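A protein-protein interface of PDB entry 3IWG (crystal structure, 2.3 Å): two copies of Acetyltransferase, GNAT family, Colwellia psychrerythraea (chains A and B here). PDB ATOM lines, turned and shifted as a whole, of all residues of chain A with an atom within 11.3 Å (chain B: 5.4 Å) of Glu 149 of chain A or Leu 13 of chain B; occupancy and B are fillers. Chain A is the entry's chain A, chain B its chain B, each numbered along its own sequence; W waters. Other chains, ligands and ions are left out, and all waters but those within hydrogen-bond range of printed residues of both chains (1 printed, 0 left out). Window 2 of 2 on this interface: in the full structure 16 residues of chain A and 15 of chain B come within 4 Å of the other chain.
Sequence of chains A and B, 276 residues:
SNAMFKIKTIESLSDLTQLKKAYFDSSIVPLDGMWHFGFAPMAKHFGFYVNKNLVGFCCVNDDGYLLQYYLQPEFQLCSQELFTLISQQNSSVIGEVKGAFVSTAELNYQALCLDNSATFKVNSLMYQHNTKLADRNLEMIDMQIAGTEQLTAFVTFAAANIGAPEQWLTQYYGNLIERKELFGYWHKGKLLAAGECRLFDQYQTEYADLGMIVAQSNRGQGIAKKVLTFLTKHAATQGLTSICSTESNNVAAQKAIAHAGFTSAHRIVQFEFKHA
Water W1 lies within hydrogen-bond range of the backbone NH of Thr 152 of chain A (2.9 Å) and the backbone carbonyl oxygen of Pro 41 of chain B (3.5 Å).
No position is printed for both chains.
Of the 5 pairs that touch across the chains among the printed residues, none has its exchanged pair printed and touching as well.
O of Glu 149 of chain A touches CB of Leu 13 of chain B, 3.4 Å away.
Thr 152 of chain A touches Pro 41 of chain B.
Among the printed residues, 5 pairs touch across the chains.
Among the printed residues, no Asp or Glu carboxylate lies within 4 Å of a Lys or Arg side-chain nitrogen of the other chain.
The side-chain hydroxyl (OG) of Ser 14 of chain B is in hydrogen-bond range of the side-chain carboxylate (OE1) of Glu 149 of chain A.
OE2 of Glu 149 of chain A lies within hydrogen-bond range of OG1 of Thr 17 of chain B, at 2.4 Å.
OE1 of Glu 11 of chain B lies close to O of Gly 189 of chain A (3.3 Å).
Of the printed residues of chain B, Thr 152 of chain A touches Pro 41.
Leu 182 of chain A touches none of the printed residues of chain B.
Of the printed residues of chain B, Gly 189 of chain A touches Glu 11 (3.3 Å).
No residue of chain A comes within 4 Å of Ile 10 of chain B.
Of the printed residues of chain A, Glu 11 of chain B touches Gly 189.
No residue of chain A comes within 4 Å of Ser 12 of chain B.
Leu 13 of chain B touches just one residue of chain A: Glu 149.
No residue of chain A comes within 4 Å of Asp 15 of chain B.
Thr 17 of chain B touches one residue of chain A.
Pro 41 of chain B touches just one residue of chain A: Thr 152.
The nearest residue of chain A that does not touch Leu 13 of chain B is Thr 152 of chain A (4.1 Å).
The nearest printed residue of chain A that does not touch Glu 11 of chain B is Lys 190 of chain A (4.5 Å).
The side-chain hydroxyl (OG1) of Thr 156 of chain A is in hydrogen-bond range of the backbone carbonyl oxygen (O) of Thr 152 of chain A (2.9 Å).
The backbone carbonyl oxygen (O) of Ser 14 of chain B sits at hydrogen-bond distance from the side-chain hydroxyl (OG1) of Thr 17 of chain B (3.2 Å).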
ATOM      1  N   GLN A 144     -15.104  -5.275  -6.132  1.00  0.00           N
ATOM      2  CA  GLN A 144     -14.618  -5.292  -7.507  1.00  0.00           C
ATOM      3  C   GLN A 144     -13.283  -6.057  -7.616  1.00  0.00           C
ATOM      4  O   GLN A 144     -12.400  -5.927  -6.789  1.00  0.00           O
ATOM      5  CB  GLN A 144     -14.560  -3.873  -8.089  1.00  0.00           C
ATOM      6  CG  GLN A 144     -13.305  -3.062  -7.718  1.00  0.00           C
ATOM      7  CD  GLN A 144     -13.279  -1.593  -8.265  1.00  0.00           C
ATOM      8  OE1 GLN A 144     -12.493  -1.282  -9.176  1.00  0.00           O
ATOM      9  NE2 GLN A 144     -14.108  -0.686  -7.673  1.00  0.00           N
ATOM     10  N   ILE A 145     -13.167  -6.903  -8.637  1.00  0.00           N
ATOM     11  CA  ILE A 145     -11.981  -7.740  -8.779  1.00  0.00           C
ATOM     12  C   ILE A 145     -10.790  -6.815  -9.002  1.00  0.00           C
ATOM     13  O   ILE A 145     -10.949  -5.806  -9.664  1.00  0.00           O
ATOM     14  CB  ILE A 145     -12.141  -8.745  -9.917  1.00  0.00           C
ATOM     15  CG1 ILE A 145     -11.035  -9.802  -9.827  1.00  0.00           C
ATOM     16  CG2 ILE A 145     -12.152  -8.033 -11.293  1.00  0.00           C
ATOM     17  CD1 ILE A 145     -11.186 -10.883 -10.813  1.00  0.00           C
ATOM     18  N   ALA A 146      -9.637  -7.097  -8.389  1.00  0.00           N
ATOM     19  CA  ALA A 146      -8.481  -6.204  -8.573  1.00  0.00           C
ATOM     20  C   ALA A 146      -7.883  -6.363  -9.988  1.00  0.00           C
ATOM     21  O   ALA A 146      -7.814  -7.443 -10.556  1.00  0.00           O
ATOM     22  CB  ALA A 146      -7.417  -6.431  -7.522  1.00  0.00           C
ATOM     23  N   GLY A 147      -7.509  -5.232 -10.556  1.00  0.00           N
ATOM     24  CA  GLY A 147      -6.763  -5.186 -11.802  1.00  0.00           C
ATOM     25  C   GLY A 147      -5.363  -4.664 -11.501  1.00  0.00           C
ATOM     26  O   GLY A 147      -5.082  -4.096 -10.431  1.00  0.00           O
ATOM     27  N   THR A 148      -4.515  -4.831 -12.501  1.00  0.00           N
ATOM     28  CA  THR A 148      -3.098  -4.562 -12.438  1.00  0.00           C
ATOM     29  C   THR A 148      -2.873  -3.157 -11.969  1.00  0.00           C
ATOM     30  O   THR A 148      -2.048  -2.927 -11.113  1.00  0.00           O
ATOM     31  CB  THR A 148      -2.501  -4.800 -13.839  1.00  0.00           C
ATOM     32  OG1 THR A 148      -2.939  -6.094 -14.308  1.00  0.00           O
ATOM     33  CG2 THR A 148      -0.988  -4.760 -13.806  1.00  0.00           C
ATOM     34  N   GLU A 149      -3.672  -2.233 -12.482  1.00  0.00           N
ATOM     35  CA  GLU A 149      -3.533  -0.825 -12.142  1.00  0.00           C
ATOM     36  C   GLU A 149      -3.640  -0.511 -10.652  1.00  0.00           C
ATOM     37  O   GLU A 149      -3.059   0.459 -10.179  1.00  0.00           O
ATOM     38  CB  GLU A 149      -4.520   0.028 -12.966  1.00  0.00           C
ATOM     39  CG  GLU A 149      -4.215  -0.039 -14.508  1.00  0.00           C
ATOM     40  CD  GLU A 149      -5.141   0.857 -15.379  1.00  0.00           C
ATOM     41  OE1 GLU A 149      -6.265   1.182 -14.905  1.00  0.00           O
ATOM     42  OE2 GLU A 149      -4.751   1.233 -16.533  1.00  0.00           O
ATOM     43  N   GLN A 150      -4.346  -1.352  -9.906  1.00  0.00           N
ATOM     44  CA  GLN A 150      -4.611  -1.098  -8.503  1.00  0.00           C
ATOM     45  C   GLN A 150      -3.633  -1.830  -7.568  1.00  0.00           C
ATOM     46  O   GLN A 150      -3.789  -1.783  -6.345  1.00  0.00           O
ATOM     47  CB  GLN A 150      -6.055  -1.552  -8.178  1.00  0.00           C
ATOM     48  CG  GLN A 150      -7.133  -0.980  -9.117  1.00  0.00           C
ATOM     49  CD  GLN A 150      -8.507  -1.635  -8.942  1.00  0.00           C
ATOM     50  OE1 GLN A 150      -8.607  -2.835  -8.802  1.00  0.00           O
ATOM     51  NE2 GLN A 150      -9.559  -0.837  -8.932  1.00  0.00           N
ATOM     52  N   LEU A 151      -2.627  -2.509  -8.110  1.00  0.00           N
ATOM     53  CA  LEU A 151      -1.758  -3.291  -7.222  1.00  0.00           C
ATOM     54  C   LEU A 151      -1.182  -2.439  -6.130  1.00  0.00           C
ATOM     55  O   LEU A 151      -1.124  -2.877  -4.976  1.00  0.00           O
ATOM     56  CB  LEU A 151      -0.629  -3.965  -8.001  1.00  0.00           C
ATOM     57  CG  LEU A 151       0.460  -4.793  -7.311  1.00  0.00           C
ATOM     58  CD1 LEU A 151      -0.066  -6.039  -6.575  1.00  0.00           C
ATOM     59  CD2 LEU A 151       1.506  -5.217  -8.404  1.00  0.00           C
ATOM     60  N   THR A 152      -0.744  -1.222  -6.473  1.00  0.00           N
ATOM     61  CA  THR A 152       0.001  -0.427  -5.490  1.00  0.00           C
ATOM     62  C   THR A 152      -0.935  -0.014  -4.356  1.00  0.00           C
ATOM     63  O   THR A 152      -0.518   0.074  -3.190  1.00  0.00           O
ATOM     64  CB  THR A 152       0.737   0.871  -6.050  1.00  0.00           C
ATOM     65  OG1 THR A 152       1.319   1.575  -4.923  1.00  0.00           O
ATOM     66  CG2 THR A 152      -0.249   1.859  -6.744  1.00  0.00           C
ATOM     67  N   ALA A 153      -2.185   0.267  -4.697  1.00  0.00           N
ATOM     68  CA  ALA A 153      -3.148   0.641  -3.675  1.00  0.00           C
ATOM     69  C   ALA A 153      -3.383  -0.545  -2.730  1.00  0.00           C
ATOM     70  O   ALA A 153      -3.351  -0.392  -1.498  1.00  0.00           O
ATOM     71  CB  ALA A 153      -4.448   1.122  -4.323  1.00  0.00           C
ATOM     72  N   PHE A 154      -3.536  -1.742  -3.281  1.00  0.00           N
ATOM     73  CA  PHE A 154      -3.651  -2.907  -2.406  1.00  0.00           C
ATOM     74  C   PHE A 154      -2.422  -3.091  -1.510  1.00  0.00           C
ATOM     75  O   PHE A 154      -2.526  -3.405  -0.327  1.00  0.00           O
ATOM     76  CB  PHE A 154      -3.935  -4.146  -3.229  1.00  0.00           C
ATOM     77  CG  PHE A 154      -5.398  -4.312  -3.605  1.00  0.00           C
ATOM     78  CD1 PHE A 154      -6.307  -4.927  -2.736  1.00  0.00           C
ATOM     79  CD2 PHE A 154      -5.868  -3.868  -4.812  1.00  0.00           C
ATOM     80  CE1 PHE A 154      -7.659  -5.084  -3.118  1.00  0.00           C
ATOM     81  CE2 PHE A 154      -7.203  -4.016  -5.181  1.00  0.00           C
ATOM     82  CZ  PHE A 154      -8.105  -4.616  -4.345  1.00  0.00           C
ATOM     83  N   VAL A 155      -1.241  -2.913  -2.081  1.00  0.00           N
ATOM     84  CA  VAL A 155       0.031  -3.124  -1.346  1.00  0.00           C
ATOM     85  C   VAL A 155       0.156  -2.128  -0.211  1.00  0.00           C
ATOM     86  O   VAL A 155       0.404  -2.500   0.946  1.00  0.00           O
ATOM     87  CB  VAL A 155       1.257  -3.059  -2.301  1.00  0.00           C
ATOM     88  CG1 VAL A 155       2.572  -2.780  -1.550  1.00  0.00           C
ATOM     89  CG2 VAL A 155       1.334  -4.378  -3.161  1.00  0.00           C
ATOM     90  N   THR A 156      -0.081  -0.872  -0.528  1.00  0.00           N
ATOM     91  CA  THR A 156      -0.122   0.154   0.489  1.00  0.00           C
ATOM     92  C   THR A 156      -1.179  -0.128   1.561  1.00  0.00           C
ATOM     93  O   THR A 156      -0.914  -0.012   2.765  1.00  0.00           O
ATOM     94  CB  THR A 156      -0.467   1.488  -0.163  1.00  0.00           C
ATOM     95  OG1 THR A 156       0.547   1.799  -1.114  1.00  0.00           O
ATOM     96  CG2 THR A 156      -0.562   2.575   0.872  1.00  0.00           C
ATOM     97  N   THR A 170       4.031  -6.923  -3.028  1.00  0.00           N
ATOM     98  CA  THR A 170       3.970  -6.625  -4.447  1.00  0.00           C
ATOM     99  C   THR A 170       3.959  -7.914  -5.252  1.00  0.00           C
ATOM    100  O   THR A 170       3.200  -8.061  -6.229  1.00  0.00           O
ATOM    101  CB  THR A 170       5.146  -5.706  -4.882  1.00  0.00           C
ATOM    102  OG1 THR A 170       5.147  -4.524  -4.079  1.00  0.00           O
ATOM    103  CG2 THR A 170       5.041  -5.302  -6.365  1.00  0.00           C
ATOM    104  N   TYR A 173       0.533 -10.170  -4.102  1.00  0.00           N
ATOM    105  CA  TYR A 173      -0.633  -9.570  -4.695  1.00  0.00           C
ATOM    106  C   TYR A 173      -0.573  -9.540  -6.209  1.00  0.00           C
ATOM    107  O   TYR A 173      -1.566  -9.757  -6.842  1.00  0.00           O
ATOM    108  CB  TYR A 173      -0.877  -8.187  -4.107  1.00  0.00           C
ATOM    109  CG  TYR A 173      -1.559  -8.125  -2.766  1.00  0.00           C
ATOM    110  CD1 TYR A 173      -2.435  -9.122  -2.322  1.00  0.00           C
ATOM    111  CD2 TYR A 173      -1.429  -6.980  -1.977  1.00  0.00           C
ATOM    112  CE1 TYR A 173      -3.102  -8.993  -1.083  1.00  0.00           C
ATOM    113  CE2 TYR A 173      -2.110  -6.835  -0.745  1.00  0.00           C
ATOM    114  CZ  TYR A 173      -2.940  -7.833  -0.320  1.00  0.00           C
ATOM    115  OH  TYR A 173      -3.584  -7.631   0.869  1.00  0.00           O
ATOM    116  N   GLY A 174       0.601  -9.364  -6.803  1.00  0.00           N
ATOM    117  CA  GLY A 174       0.698  -9.417  -8.277  1.00  0.00           C
ATOM    118  C   GLY A 174       0.237 -10.760  -8.806  1.00  0.00           C
ATOM    119  O   GLY A 174      -0.521 -10.895  -9.773  1.00  0.00           O
ATOM    120  N   LEU A 176      -1.757 -12.847  -7.113  1.00  0.00           N
ATOM    121  CA  LEU A 176      -3.202 -13.065  -6.908  1.00  0.00           C
ATOM    122  C   LEU A 176      -4.041 -12.372  -7.997  1.00  0.00           C
ATOM    123  O   LEU A 176      -5.045 -12.904  -8.464  1.00  0.00           O
ATOM    124  CB  LEU A 176      -3.623 -12.607  -5.536  1.00  0.00           C
ATOM    125  CG  LEU A 176      -3.757 -13.552  -4.320  1.00  0.00           C
ATOM    126  CD1 LEU A 176      -2.898 -14.801  -4.290  1.00  0.00           C
ATOM    127  CD2 LEU A 176      -3.587 -12.747  -3.053  1.00  0.00           C
ATOM    128  N   ILE A 177      -3.604 -11.192  -8.418  1.00  0.00           N
ATOM    129  CA  ILE A 177      -4.294 -10.423  -9.422  1.00  0.00           C
ATOM    130  C   ILE A 177      -4.362 -11.238 -10.713  1.00  0.00           C
ATOM    131  O   ILE A 177      -5.442 -11.357 -11.317  1.00  0.00           O
ATOM    132  CB  ILE A 177      -3.576  -9.103  -9.649  1.00  0.00           C
ATOM    133  CG1 ILE A 177      -3.908  -8.114  -8.521  1.00  0.00           C
ATOM    134  CG2 ILE A 177      -3.924  -8.536 -11.049  1.00  0.00           C
ATOM    135  CD1 ILE A 177      -3.296  -6.797  -8.673  1.00  0.00           C
ATOM    136  N   GLU A 178      -3.236 -11.850 -11.100  1.00  0.00           N
ATOM    137  CA  GLU A 178      -3.179 -12.682 -12.307  1.00  0.00           C
ATOM    138  C   GLU A 178      -4.046 -13.888 -12.181  1.00  0.00           C
ATOM    139  O   GLU A 178      -4.637 -14.340 -13.179  1.00  0.00           O
ATOM    140  CB  GLU A 178      -1.760 -13.172 -12.581  1.00  0.00           C
ATOM    141  CG  GLU A 178      -0.786 -12.003 -12.922  1.00  0.00           C
ATOM    142  CD  GLU A 178       0.568 -12.519 -13.424  1.00  0.00           C
ATOM    143  OE1 GLU A 178       0.558 -13.417 -14.298  1.00  0.00           O
ATOM    144  OE2 GLU A 178       1.611 -12.010 -12.955  1.00  0.00           O
ATOM    145  N   LEU A 182      -8.082 -11.727  -6.036  1.00  0.00           N
ATOM    146  CA  LEU A 182      -8.068 -10.599  -5.105  1.00  0.00           C
ATOM    147  C   LEU A 182      -9.230  -9.666  -5.385  1.00  0.00           C
ATOM    148  O   LEU A 182      -9.509  -9.378  -6.538  1.00  0.00           O
ATOM    149  CB  LEU A 182      -6.736  -9.853  -5.190  1.00  0.00           C
ATOM    150  CG  LEU A 182      -6.466  -8.612  -4.288  1.00  0.00           C
ATOM    151  CD1 LEU A 182      -6.453  -8.931  -2.812  1.00  0.00           C
ATOM    152  CD2 LEU A 182      -5.128  -7.960  -4.714  1.00  0.00           C
ATOM    153  N   TRP A 186     -14.463  -0.727  -1.971  1.00  0.00           N
ATOM    154  CA  TRP A 186     -14.038   0.647  -2.195  1.00  0.00           C
ATOM    155  C   TRP A 186     -15.101   1.622  -1.782  1.00  0.00           C
ATOM    156  O   TRP A 186     -16.315   1.362  -1.873  1.00  0.00           O
ATOM    157  CB  TRP A 186     -13.779   0.896  -3.700  1.00  0.00           C
ATOM    158  CG  TRP A 186     -12.637   0.128  -4.254  1.00  0.00           C
ATOM    159  CD1 TRP A 186     -12.668  -1.116  -4.774  1.00  0.00           C
ATOM    160  CD2 TRP A 186     -11.297   0.569  -4.348  1.00  0.00           C
ATOM    161  NE1 TRP A 186     -11.426  -1.484  -5.202  1.00  0.00           N
ATOM    162  CE2 TRP A 186     -10.560  -0.459  -4.945  1.00  0.00           C
ATOM    163  CE3 TRP A 186     -10.645   1.755  -4.008  1.00  0.00           C
ATOM    164  CZ2 TRP A 186      -9.189  -0.348  -5.198  1.00  0.00           C
ATOM    165  CZ3 TRP A 186      -9.283   1.873  -4.282  1.00  0.00           C
ATOM    166  CH2 TRP A 186      -8.578   0.832  -4.858  1.00  0.00           C
ATOM    167  N   GLY A 189     -12.949   6.324  -3.875  1.00  0.00           N
ATOM    168  CA  GLY A 189     -11.553   6.108  -4.237  1.00  0.00           C
ATOM    169  C   GLY A 189     -10.639   5.440  -3.196  1.00  0.00           C
ATOM    170  O   GLY A 189      -9.437   5.320  -3.419  1.00  0.00           O
ATOM    171  N   LYS A 190     -11.172   4.986  -2.066  1.00  0.00           N
ATOM    172  CA  LYS A 190     -10.329   4.318  -1.053  1.00  0.00           C
ATOM    173  C   LYS A 190     -10.819   2.904  -0.685  1.00  0.00           C
ATOM    174  O   LYS A 190     -12.006   2.571  -0.804  1.00  0.00           O
ATOM    175  CB  LYS A 190     -10.219   5.199   0.210  1.00  0.00           C
ATOM    176  CG  LYS A 190      -9.206   6.337   0.091  1.00  0.00           C
ATOM    177  CD  LYS A 190      -9.448   7.429   1.153  1.00  0.00           C
ATOM    178  CE  LYS A 190      -8.400   8.584   1.028  1.00  0.00           C
ATOM    179  NZ  LYS A 190      -7.064   8.239   1.712  1.00  0.00           N
ATOM    180  N   LEU A 191      -9.865   2.095  -0.243  1.00  0.00           N
ATOM    181  CA  LEU A 191     -10.088   0.706   0.077  1.00  0.00           C
ATOM    182  C   LEU A 191     -10.646   0.609   1.490  1.00  0.00           C
ATOM    183  O   LEU A 191      -9.997   1.055   2.410  1.00  0.00           O
ATOM    184  CB  LEU A 191      -8.768  -0.076  -0.007  1.00  0.00           C
ATOM    185  CG  LEU A 191      -8.518  -0.749  -1.350  1.00  0.00           C
ATOM    186  CD1 LEU A 191      -7.169  -1.472  -1.335  1.00  0.00           C
ATOM    187  CD2 LEU A 191      -9.687  -1.749  -1.703  1.00  0.00           C
ATOM    188  N   ILE B  10      -2.007  11.647  -8.016  1.00  0.00           N
ATOM    189  CA  ILE B  10      -2.932  10.710  -8.674  1.00  0.00           C
ATOM    190  C   ILE B  10      -3.402   9.594  -7.741  1.00  0.00           C
ATOM    191  O   ILE B  10      -2.612   8.719  -7.355  1.00  0.00           O
ATOM    192  CB  ILE B  10      -2.287  10.011  -9.880  1.00  0.00           C
ATOM    193  CG1 ILE B  10      -1.919  11.046 -10.987  1.00  0.00           C
ATOM    194  CG2 ILE B  10      -3.201   8.883 -10.365  1.00  0.00           C
ATOM    195  CD1 ILE B  10      -3.043  11.457 -11.909  1.00  0.00           C
ATOM    196  N   GLU B  11      -4.694   9.626  -7.410  1.00  0.00           N
ATOM    197  CA  GLU B  11      -5.323   8.613  -6.554  1.00  0.00           C
ATOM    198  C   GLU B  11      -5.204   7.253  -7.207  1.00  0.00           C
ATOM    199  O   GLU B  11      -4.520   6.378  -6.711  1.00  0.00           O
ATOM    200  CB  GLU B  11      -6.810   8.923  -6.351  1.00  0.00           C
ATOM    201  CG  GLU B  11      -7.148   9.683  -5.091  1.00  0.00           C
ATOM    202  CD  GLU B  11      -7.800   8.795  -4.016  1.00  0.00           C
ATOM    203  OE1 GLU B  11      -7.177   7.782  -3.623  1.00  0.00           O
ATOM    204  OE2 GLU B  11      -8.930   9.119  -3.573  1.00  0.00           O
ATOM    205  N   SER B  12      -5.864   7.093  -8.346  1.00  0.00           N
ATOM    206  CA  SER B  12      -5.982   5.789  -8.964  1.00  0.00           C
ATOM    207  C   SER B  12      -5.233   5.740 -10.293  1.00  0.00           C
ATOM    208  O   SER B  12      -5.510   6.531 -11.198  1.00  0.00           O
ATOM    209  CB  SER B  12      -7.454   5.460  -9.176  1.00  0.00           C
ATOM    210  OG  SER B  12      -7.594   4.094  -9.530  1.00  0.00           O
ATOM    211  N   LEU B  13      -4.294   4.798 -10.400  1.00  0.00           N
ATOM    212  CA  LEU B  13      -3.506   4.624 -11.612  1.00  0.00           C
ATOM    213  C   LEU B  13      -4.336   4.309 -12.861  1.00  0.00           C
ATOM    214  O   LEU B  13      -3.883   4.516 -13.972  1.00  0.00           O
ATOM    215  CB  LEU B  13      -2.409   3.568 -11.401  1.00  0.00           C
ATOM    216  CG  LEU B  13      -1.040   4.109 -10.957  1.00  0.00           C
ATOM    217  CD1 LEU B  13      -1.211   5.028  -9.739  1.00  0.00           C
ATOM    218  CD2 LEU B  13      -0.053   2.966 -10.686  1.00  0.00           C
ATOM    219  N   SER B  14      -5.550   3.820 -12.678  1.00  0.00           N
ATOM    220  CA  SER B  14      -6.538   3.738 -13.770  1.00  0.00           C
ATOM    221  C   SER B  14      -6.891   5.048 -14.497  1.00  0.00           C
ATOM    222  O   SER B  14      -7.426   4.994 -15.599  1.00  0.00           O
ATOM    223  CB  SER B  14      -7.842   3.118 -13.259  1.00  0.00           C
ATOM    224  OG  SER B  14      -7.576   1.891 -12.593  1.00  0.00           O
ATOM    225  N   ASP B  15      -6.621   6.205 -13.893  1.00  0.00           N
ATOM    226  CA  ASP B  15      -6.793   7.498 -14.594  1.00  0.00           C
ATOM    227  C   ASP B  15      -5.709   7.710 -15.689  1.00  0.00           C
ATOM    228  O   ASP B  15      -5.911   8.468 -16.638  1.00  0.00           O
ATOM    229  CB  ASP B  15      -6.778   8.684 -13.595  1.00  0.00           C
ATOM    230  CG  ASP B  15      -7.937   8.649 -12.565  1.00  0.00           C
ATOM    231  OD1 ASP B  15      -8.980   7.987 -12.791  1.00  0.00           O
ATOM    232  OD2 ASP B  15      -7.799   9.302 -11.506  1.00  0.00           O
ATOM    233  N   LEU B  16      -4.567   7.034 -15.554  1.00  0.00           N
ATOM    234  CA  LEU B  16      -3.426   7.281 -16.426  1.00  0.00           C
ATOM    235  C   LEU B  16      -3.414   6.376 -17.644  1.00  0.00           C
ATOM    236  O   LEU B  16      -2.529   6.488 -18.488  1.00  0.00           O
ATOM    237  CB  LEU B  16      -2.104   7.146 -15.646  1.00  0.00           C
ATOM    238  CG  LEU B  16      -1.873   8.157 -14.503  1.00  0.00           C
ATOM    239  CD1 LEU B  16      -0.564   7.919 -13.743  1.00  0.00           C
ATOM    240  CD2 LEU B  16      -1.890   9.555 -15.036  1.00  0.00           C
ATOM    241  N   THR B  17      -4.401   5.497 -17.757  1.00  0.00           N
ATOM    242  CA  THR B  17      -4.382   4.472 -18.802  1.00  0.00           C
ATOM    243  C   THR B  17      -3.977   4.999 -20.197  1.00  0.00           C
ATOM    244  O   THR B  17      -2.969   4.565 -20.760  1.00  0.00           O
ATOM    245  CB  THR B  17      -5.737   3.753 -18.879  1.00  0.00           C
ATOM    246  OG1 THR B  17      -5.943   2.993 -17.674  1.00  0.00           O
ATOM    247  CG2 THR B  17      -5.754   2.794 -20.050  1.00  0.00           C
ATOM    248  N   PRO B  41       5.312   1.506 -11.348  1.00  0.00           N
ATOM    249  CA  PRO B  41       3.965   1.450 -10.772  1.00  0.00           C
ATOM    250  C   PRO B  41       3.904   1.637  -9.247  1.00  0.00           C
ATOM    251  O   PRO B  41       2.880   2.091  -8.769  1.00  0.00           O
ATOM    252  CB  PRO B  41       3.448   0.067 -11.183  1.00  0.00           C
ATOM    253  CG  PRO B  41       4.200  -0.255 -12.420  1.00  0.00           C
ATOM    254  CD  PRO B  41       5.585   0.347 -12.199  1.00  0.00           C
ATOM    255  N   HIS B  45       2.553   8.822  -8.082  1.00  0.00           N
ATOM    256  CA  HIS B  45       2.197   9.502  -9.332  1.00  0.00           C
ATOM    257  C   HIS B  45       1.534  10.866  -9.127  1.00  0.00           C
ATOM    258  O   HIS B  45       0.943  11.139  -8.096  1.00  0.00           O
ATOM    259  CB  HIS B  45       1.334   8.612 -10.209  1.00  0.00           C
ATOM    260  CG  HIS B  45       2.068   7.422 -10.726  1.00  0.00           C
ATOM    261  ND1 HIS B  45       2.200   7.149 -12.070  1.00  0.00           N
ATOM    262  CD2 HIS B  45       2.739   6.448 -10.079  1.00  0.00           C
ATOM    263  CE1 HIS B  45       2.922   6.053 -12.227  1.00  0.00           C
ATOM    264  NE2 HIS B  45       3.273   5.619 -11.033  1.00  0.00           N
ATOM    265  N   TYR B 203       1.525  -3.330 -23.586  1.00  0.00           N
ATOM    266  CA  TYR B 203       2.342  -2.339 -24.300  1.00  0.00           C
ATOM    267  C   TYR B 203       3.473  -2.918 -25.132  1.00  0.00           C
ATOM    268  O   TYR B 203       3.752  -2.402 -26.196  1.00  0.00           O
ATOM    269  CB  TYR B 203       2.968  -1.317 -23.343  1.00  0.00           C
ATOM    270  CG  TYR B 203       2.026  -0.686 -22.350  1.00  0.00           C
ATOM    271  CD1 TYR B 203       0.905   0.035 -22.759  1.00  0.00           C
ATOM    272  CD2 TYR B 203       2.289  -0.776 -21.002  1.00  0.00           C
ATOM    273  CE1 TYR B 203       0.074   0.625 -21.834  1.00  0.00           C
ATOM    274  CE2 TYR B 203       1.476  -0.195 -20.060  1.00  0.00           C
ATOM    275  CZ  TYR B 203       0.373   0.508 -20.470  1.00  0.00           C
ATOM    276  OH  TYR B 203      -0.423   1.062 -19.486  1.00  0.00           O
HETATM  277  O   HOH W   1       0.391  -0.329  -9.024  1.00  0.00           O
